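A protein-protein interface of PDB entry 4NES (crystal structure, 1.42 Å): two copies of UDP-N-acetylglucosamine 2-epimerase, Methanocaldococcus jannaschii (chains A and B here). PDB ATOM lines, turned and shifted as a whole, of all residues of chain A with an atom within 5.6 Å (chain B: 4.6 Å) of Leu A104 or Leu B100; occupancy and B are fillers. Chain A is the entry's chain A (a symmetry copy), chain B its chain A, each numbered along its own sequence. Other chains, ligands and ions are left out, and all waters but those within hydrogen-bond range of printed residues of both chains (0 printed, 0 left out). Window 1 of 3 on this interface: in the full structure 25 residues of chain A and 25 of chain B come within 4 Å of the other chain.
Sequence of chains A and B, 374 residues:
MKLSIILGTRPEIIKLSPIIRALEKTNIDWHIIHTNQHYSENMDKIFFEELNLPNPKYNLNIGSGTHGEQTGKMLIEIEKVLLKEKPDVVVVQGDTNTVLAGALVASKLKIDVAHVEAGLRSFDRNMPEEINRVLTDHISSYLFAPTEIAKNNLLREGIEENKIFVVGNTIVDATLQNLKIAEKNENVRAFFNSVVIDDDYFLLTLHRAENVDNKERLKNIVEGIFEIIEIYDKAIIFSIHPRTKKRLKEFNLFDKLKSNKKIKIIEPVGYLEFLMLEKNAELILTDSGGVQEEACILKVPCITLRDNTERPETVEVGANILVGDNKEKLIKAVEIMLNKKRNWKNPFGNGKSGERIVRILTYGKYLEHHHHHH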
ATOM      1  N   LEU A  75      22.395   6.450  -7.210  1.00  0.00           N
ATOM      2  CA  LEU A  75      22.009   6.139  -5.830  1.00  0.00           C
ATOM      3  C   LEU A  75      20.777   5.247  -5.809  1.00  0.00           C
ATOM      4  O   LEU A  75      20.722   4.265  -5.064  1.00  0.00           O
ATOM      5  CB  LEU A  75      21.708   7.404  -5.018  1.00  0.00           C
ATOM      6  CG  LEU A  75      22.842   8.402  -4.787  1.00  0.00           C
ATOM      7  CD1 LEU A  75      22.377   9.546  -3.886  1.00  0.00           C
ATOM      8  CD2 LEU A  75      24.052   7.718  -4.183  1.00  0.00           C
ATOM      9  N   VAL A  99      32.009   6.213  -8.282  1.00  0.00           N
ATOM     10  CA  VAL A  99      32.673   5.940  -7.009  1.00  0.00           C
ATOM     11  C   VAL A  99      31.901   6.564  -5.850  1.00  0.00           C
ATOM     12  O   VAL A  99      31.615   5.907  -4.846  1.00  0.00           O
ATOM     13  CB  VAL A  99      34.111   6.487  -7.020  1.00  0.00           C
ATOM     14  CG1 VAL A  99      34.742   6.408  -5.635  1.00  0.00           C
ATOM     15  CG2 VAL A  99      34.935   5.740  -8.047  1.00  0.00           C
ATOM     16  N   LEU A 100      31.571   7.841  -5.986  1.00  0.00           N
ATOM     17  CA  LEU A 100      30.837   8.528  -4.934  1.00  0.00           C
ATOM     18  C   LEU A 100      29.480   7.880  -4.695  1.00  0.00           C
ATOM     19  O   LEU A 100      29.096   7.650  -3.554  1.00  0.00           O
ATOM     20  CB  LEU A 100      30.657  10.004  -5.275  1.00  0.00           C
ATOM     21  CG  LEU A 100      29.803  10.779  -4.271  1.00  0.00           C
ATOM     22  CD1 LEU A 100      30.483  10.802  -2.912  1.00  0.00           C
ATOM     23  CD2 LEU A 100      29.521  12.209  -4.763  1.00  0.00           C
ATOM     24  N   ALA A 101      28.764   7.556  -5.767  1.00  0.00           N
ATOM     25  CA  ALA A 101      27.426   6.990  -5.621  1.00  0.00           C
ATOM     26  C   ALA A 101      27.501   5.634  -4.925  1.00  0.00           C
ATOM     27  O   ALA A 101      26.721   5.346  -4.019  1.00  0.00           O
ATOM     28  CB  ALA A 101      26.737   6.873  -6.967  1.00  0.00           C
ATOM     29  N   GLY A 102      28.449   4.802  -5.346  1.00  0.00           N
ATOM     30  CA  GLY A 102      28.602   3.502  -4.719  1.00  0.00           C
ATOM     31  C   GLY A 102      28.902   3.616  -3.238  1.00  0.00           C
ATOM     32  O   GLY A 102      28.318   2.892  -2.421  1.00  0.00           O
ATOM     33  N   ALA A 103      29.829   4.505  -2.890  1.00  0.00           N
ATOM     34  CA  ALA A 103      30.216   4.697  -1.488  1.00  0.00           C
ATOM     35  C   ALA A 103      29.075   5.249  -0.637  1.00  0.00           C
ATOM     36  O   ALA A 103      28.869   4.807   0.498  1.00  0.00           O
ATOM     37  CB  ALA A 103      31.438   5.608  -1.389  1.00  0.00           C
ATOM     38  N   LEU A 104      28.351   6.220  -1.180  1.00  0.00           N
ATOM     39  CA  LEU A 104      27.260   6.834  -0.452  1.00  0.00           C
ATOM     40  C   LEU A 104      26.125   5.843  -0.200  1.00  0.00           C
ATOM     41  O   LEU A 104      25.557   5.819   0.893  1.00  0.00           O
ATOM     42  CB  LEU A 104      26.759   8.066  -1.195  1.00  0.00           C
ATOM     43  CG  LEU A 104      25.686   8.865  -0.462  1.00  0.00           C
ATOM     44  CD1 LEU A 104      26.091   9.135   0.989  1.00  0.00           C
ATOM     45  CD2 LEU A 104      25.461  10.170  -1.199  1.00  0.00           C
ATOM     46  N   VAL A 105      25.794   5.020  -1.191  1.00  0.00           N
ATOM     47  CA  VAL A 105      24.759   4.016  -0.983  1.00  0.00           C
ATOM     48  C   VAL A 105      25.198   3.033   0.095  1.00  0.00           C
ATOM     49  O   VAL A 105      24.457   2.758   1.037  1.00  0.00           O
ATOM     50  CB  VAL A 105      24.424   3.229  -2.274  1.00  0.00           C
ATOM     51  CG1 VAL A 105      23.519   2.051  -1.947  1.00  0.00           C
ATOM     52  CG2 VAL A 105      23.766   4.128  -3.310  1.00  0.00           C
ATOM     53  N   ALA A 106      26.411   2.509  -0.048  1.00  0.00           N
ATOM     54  CA  ALA A 106      26.911   1.510   0.884  1.00  0.00           C
ATOM     55  C   ALA A 106      26.981   2.034   2.314  1.00  0.00           C
ATOM     56  O   ALA A 106      26.578   1.352   3.251  1.00  0.00           O
ATOM     57  CB  ALA A 106      28.264   0.983   0.430  1.00  0.00           C
ATOM     58  N   SER A 107      27.463   3.260   2.480  1.00  0.00           N
ATOM     59  CA  SER A 107      27.603   3.850   3.807  1.00  0.00           C
ATOM     60  C   SER A 107      26.273   3.940   4.551  1.00  0.00           C
ATOM     61  O   SER A 107      26.209   3.637   5.742  1.00  0.00           O
ATOM     62  CB  SER A 107      28.271   5.231   3.718  1.00  0.00           C
ATOM     63  OG  SER A 107      27.397   6.195   3.174  1.00  0.00           O
ATOM     64  N   LYS A 108      25.207   4.335   3.863  1.00  0.00           N
ATOM     65  CA  LYS A 108      23.907   4.434   4.519  1.00  0.00           C
ATOM     66  C   LYS A 108      23.292   3.063   4.796  1.00  0.00           C
ATOM     67  O   LYS A 108      22.443   2.927   5.667  1.00  0.00           O
ATOM     68  CB  LYS A 108      22.935   5.291   3.701  1.00  0.00           C
ATOM     69  CG  LYS A 108      23.327   6.771   3.593  1.00  0.00           C
ATOM     70  CD  LYS A 108      23.181   7.482   4.945  1.00  0.00           C
ATOM     71  CE  LYS A 108      23.511   8.974   4.844  1.00  0.00           C
ATOM     72  NZ  LYS A 108      22.469   9.747   4.091  1.00  0.00           N
ATOM     73  N   LEU A 109      23.728   2.043   4.054  1.00  0.00           N
ATOM     74  CA  LEU A 109      23.277   0.678   4.293  1.00  0.00           C
ATOM     75  C   LEU A 109      24.150  -0.031   5.323  1.00  0.00           C
ATOM     76  O   LEU A 109      23.920  -1.202   5.634  1.00  0.00           O
ATOM     77  CB  LEU A 109      23.281  -0.126   2.993  1.00  0.00           C
ATOM     78  CG  LEU A 109      22.238   0.238   1.931  1.00  0.00           C
ATOM     79  CD1 LEU A 109      22.379  -0.676   0.712  1.00  0.00           C
ATOM     80  CD2 LEU A 109      20.820   0.174   2.491  1.00  0.00           C
ATOM     81  N   ILE A 139      33.882   8.416   4.016  1.00  0.00           N
ATOM     82  CA  ILE A 139      32.934   7.357   4.368  1.00  0.00           C
ATOM     83  C   ILE A 139      33.495   5.959   4.121  1.00  0.00           C
ATOM     84  O   ILE A 139      32.751   4.974   4.132  1.00  0.00           O
ATOM     85  CB  ILE A 139      31.567   7.532   3.673  1.00  0.00           C
ATOM     86  CG1 ILE A 139      31.758   7.833   2.192  1.00  0.00           C
ATOM     87  CG2 ILE A 139      30.752   8.627   4.362  1.00  0.00           C
ATOM     88  CD1 ILE A 139      30.456   7.960   1.431  1.00  0.00           C
ATOM     89  N   THR B  96      20.217  16.301   7.831  1.00  0.00           N
ATOM     90  CA  THR B  96      19.249  15.385   7.239  1.00  0.00           C
ATOM     91  C   THR B  96      19.680  15.017   5.825  1.00  0.00           C
ATOM     92  O   THR B  96      20.609  15.611   5.276  1.00  0.00           O
ATOM     93  CB  THR B  96      17.853  16.020   7.197  1.00  0.00           C
ATOM     94  OG1 THR B  96      17.884  17.135   6.297  1.00  0.00           O
ATOM     95  CG2 THR B  96      17.445  16.506   8.585  1.00  0.00           C
ATOM     96  N   ASN B  97      18.998  14.048   5.223  1.00  0.00           N
ATOM     97  CA  ASN B  97      19.286  13.710   3.829  1.00  0.00           C
ATOM     98  C   ASN B  97      19.071  14.898   2.889  1.00  0.00           C
ATOM     99  O   ASN B  97      19.779  15.038   1.897  1.00  0.00           O
ATOM    100  CB  ASN B  97      18.473  12.503   3.361  1.00  0.00           C
ATOM    101  CG  ASN B  97      18.987  11.199   3.927  1.00  0.00           C
ATOM    102  OD1 ASN B  97      20.057  11.143   4.537  1.00  0.00           O
ATOM    103  ND2 ASN B  97      18.227  10.129   3.715  1.00  0.00           N
ATOM    104  N   THR B  98      18.107  15.755   3.219  1.00  0.00           N
ATOM    105  CA  THR B  98      17.874  16.964   2.448  1.00  0.00           C
ATOM    106  C   THR B  98      19.116  17.853   2.418  1.00  0.00           C
ATOM    107  O   THR B  98      19.470  18.399   1.369  1.00  0.00           O
ATOM    108  CB  THR B  98      16.685  17.744   3.019  1.00  0.00           C
ATOM    109  OG1 THR B  98      15.475  17.031   2.720  1.00  0.00           O
ATOM    110  CG2 THR B  98      16.621  19.134   2.409  1.00  0.00           C
ATOM    111  N   VAL B  99      19.789  17.980   3.561  1.00  0.00           N
ATOM    112  CA  VAL B  99      20.991  18.803   3.667  1.00  0.00           C
ATOM    113  C   VAL B  99      22.091  18.276   2.750  1.00  0.00           C
ATOM    114  O   VAL B  99      22.698  19.028   1.983  1.00  0.00           O
ATOM    115  CB  VAL B  99      21.503  18.833   5.117  1.00  0.00           C
ATOM    116  CG1 VAL B  99      22.870  19.501   5.207  1.00  0.00           C
ATOM    117  CG2 VAL B  99      20.490  19.523   6.005  1.00  0.00           C
ATOM    118  N   LEU B 100      22.356  16.980   2.838  1.00  0.00           N
ATOM    119  CA  LEU B 100      23.392  16.382   2.009  1.00  0.00           C
ATOM    120  C   LEU B 100      23.067  16.534   0.528  1.00  0.00           C
ATOM    121  O   LEU B 100      23.929  16.905  -0.260  1.00  0.00           O
ATOM    122  CB  LEU B 100      23.576  14.907   2.353  1.00  0.00           C
ATOM    123  CG  LEU B 100      24.573  14.175   1.454  1.00  0.00           C
ATOM    124  CD1 LEU B 100      25.964  14.763   1.624  1.00  0.00           C
ATOM    125  CD2 LEU B 100      24.582  12.664   1.744  1.00  0.00           C
ATOM    126  N   ALA B 101      21.819  16.277   0.150  1.00  0.00           N
ATOM    127  CA  ALA B 101      21.445  16.337  -1.260  1.00  0.00           C
ATOM    128  C   ALA B 101      21.601  17.761  -1.785  1.00  0.00           C
ATOM    129  O   ALA B 101      22.140  17.979  -2.869  1.00  0.00           O
ATOM    130  CB  ALA B 101      20.030  15.833  -1.468  1.00  0.00           C
ATOM    131  N   GLY B 102      21.132  18.735  -1.011  1.00  0.00           N
ATOM    132  CA  GLY B 102      21.263  20.119  -1.428  1.00  0.00           C
ATOM    133  C   GLY B 102      22.711  20.521  -1.618  1.00  0.00           C
ATOM    134  O   GLY B 102      23.057  21.175  -2.611  1.00  0.00           O
ATOM    135  N   ALA B 103      23.558  20.156  -0.657  1.00  0.00           N
ATOM    136  CA  ALA B 103      24.982  20.500  -0.722  1.00  0.00           C
ATOM    137  C   ALA B 103      25.694  19.821  -1.890  1.00  0.00           C
ATOM    138  O   ALA B 103      26.515  20.445  -2.571  1.00  0.00           O
ATOM    139  CB  ALA B 103      25.676  20.155   0.594  1.00  0.00           C
ATOM    140  N   LEU B 104      25.392  18.546  -2.104  1.00  0.00           N
ATOM    141  CA  LEU B 104      26.027  17.797  -3.169  1.00  0.00           C
ATOM    142  C   LEU B 104      25.640  18.339  -4.544  1.00  0.00           C
ATOM    143  O   LEU B 104      26.493  18.447  -5.427  1.00  0.00           O
ATOM    144  CB  LEU B 104      25.687  16.318  -3.046  1.00  0.00           C
ATOM    145  CG  LEU B 104      26.399  15.412  -4.047  1.00  0.00           C
ATOM    146  CD1 LEU B 104      27.900  15.705  -4.090  1.00  0.00           C
ATOM    147  CD2 LEU B 104      26.154  13.968  -3.657  1.00  0.00           C
ATOM    148  N   ILE B 131      27.181  10.953   8.947  1.00  0.00           N
ATOM    149  CA  ILE B 131      27.627  10.898   7.552  1.00  0.00           C
ATOM    150  C   ILE B 131      27.219  12.167   6.824  1.00  0.00           C
ATOM    151  O   ILE B 131      28.047  12.820   6.190  1.00  0.00           O
ATOM    152  CB  ILE B 131      27.067   9.667   6.814  1.00  0.00           C
ATOM    153  CG1 ILE B 131      27.732   8.389   7.340  1.00  0.00           C
ATOM    154  CG2 ILE B 131      27.300   9.786   5.317  1.00  0.00           C
ATOM    155  CD1 ILE B 131      26.984   7.113   6.989  1.00  0.00           C
ATOM    156  N   ASN B 132      25.948  12.545   6.951  1.00  0.00           N
ATOM    157  CA  ASN B 132      25.436  13.713   6.249  1.00  0.00           C
ATOM    158  C   ASN B 132      26.188  14.975   6.632  1.00  0.00           C
ATOM    159  O   ASN B 132      26.547  15.792   5.782  1.00  0.00           O
ATOM    160  CB  ASN B 132      23.947  13.906   6.530  1.00  0.00           C
ATOM    161  CG  ASN B 132      23.083  12.866   5.849  1.00  0.00           C
ATOM    162  OD1 ASN B 132      23.511  12.224   4.886  1.00  0.00           O
ATOM    163  ND2 ASN B 132      21.855  12.687   6.350  1.00  0.00           N
ATOM    164  N   LEU B 135      30.045  14.915   5.446  1.00  0.00           N
ATOM    165  CA  LEU B 135      30.161  15.121   4.007  1.00  0.00           C
ATOM    166  C   LEU B 135      29.818  16.554   3.620  1.00  0.00           C
ATOM    167  O   LEU B 135      30.537  17.204   2.857  1.00  0.00           O
ATOM    168  CB  LEU B 135      29.273  14.136   3.250  1.00  0.00           C
ATOM    169  CG  LEU B 135      29.668  12.667   3.417  1.00  0.00           C
ATOM    170  CD1 LEU B 135      28.819  11.803   2.506  1.00  0.00           C
ATOM    171  CD2 LEU B 135      31.140  12.445   3.129  1.00  0.00           C
ATOM    172  N   THR B 136      28.730  17.070   4.190  1.00  0.00           N
ATOM    173  CA  THR B 136      28.311  18.432   3.897  1.00  0.00           C
ATOM    174  C   THR B 136      29.386  19.435   4.307  1.00  0.00           C
ATOM    175  O   THR B 136      29.681  20.376   3.553  1.00  0.00           O
ATOM    176  CB  THR B 136      26.989  18.760   4.600  1.00  0.00           C
ATOM    177  OG1 THR B 136      25.955  17.919   4.072  1.00  0.00           O
ATOM    178  CG2 THR B 136      26.606  20.205   4.365  1.00  0.00           C
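NZ of Lys A108 lies within hydrogen-bond range of OD1 of Asn B97, at 2.8 Å.
OD1 of Asn B132 lies within hydrogen-bond range of NZ of Lys A108 (2.8 Å).
O of Thr B96 sits close to ND2 of Asn B132 (3.4 Å).
The side-chain amide oxygen (OD1) of Asn B97 lies within hydrogen-bond range of the side-chain amide nitrogen (ND2) of Asn B132, at 3.0 Å.
The backbone carbonyl oxygen of Asn B132 is in hydrogen-bond range of the side-chain hydroxyl of Thr B136 (2.8 Å).
The side-chain hydroxyl of Ser A107 lies close to the backbone carbonyl oxygen of Ala A103 (3.4 Å).
O of Leu A104 sits at hydrogen-bond distance from OG of Ser A107 (3.0 Å).
Among the printed residues, merely in contact across the chains: Ile A139 with Ile B131 (3.8 Å), Ser A107 with Ile B131 (3.8 Å), Lys A108 with Ile B131 (3.9 Å), Leu A104 with Leu B100 (3.9 Å) and Leu A100 with Leu B104 (3.9 Å).
Leu A104 touches just one residue of chain B: Leu B100 (3.9 Å).
Of chain A, only Leu A104 comes within 4 Å of Leu B100.
Printed residues of chain A within 4 Å of Ile B131: Ser A107, Lys A108 and Ile A139.
Printed residues of chain B within 4 Å of Lys A108: Asn B97 (2.8 Å), Ile B131 (3.9 Å) and Asn B132 (2.8 Å).
Of the printed residues of chain B, Ser A107 touches Ile B131.
Of the printed residues of chain A, Asn B132 touches Lys A108.
Printed residues of chain A within 4 Å of Leu B104: Leu A100 (3.9 Å).
Leu B135 touches none of the printed residues of chain A.
The nearest residue of chain B that does not touch Leu A104 is Leu B135 (4.1 Å).
The nearest residue of chain A that does not touch Leu B100 is Lys A108 (4.3 Å).
The nearest printed residue of chain A that does not touch Leu B104 is Leu A104 (4.6 Å).
Hydrophobic or aromatic side chains of chain A that line the printed part of chain B: Leu A100, Leu A104 and Ile A139.
Hydrophobic or aromatic side chains of chain B that line the printed part of chain A: Leu B100, Leu B104 and Ile B131.
Among the printed residues, 7 pairs touch across the chains.
Among the printed residues, no Asp or Glu carboxylate lies within 4 Å of a Lys or Arg side-chain nitrogen of the other chain.
Leu A100 touches Leu B104, and with the chains exchanged Leu A104 touches Leu B100.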
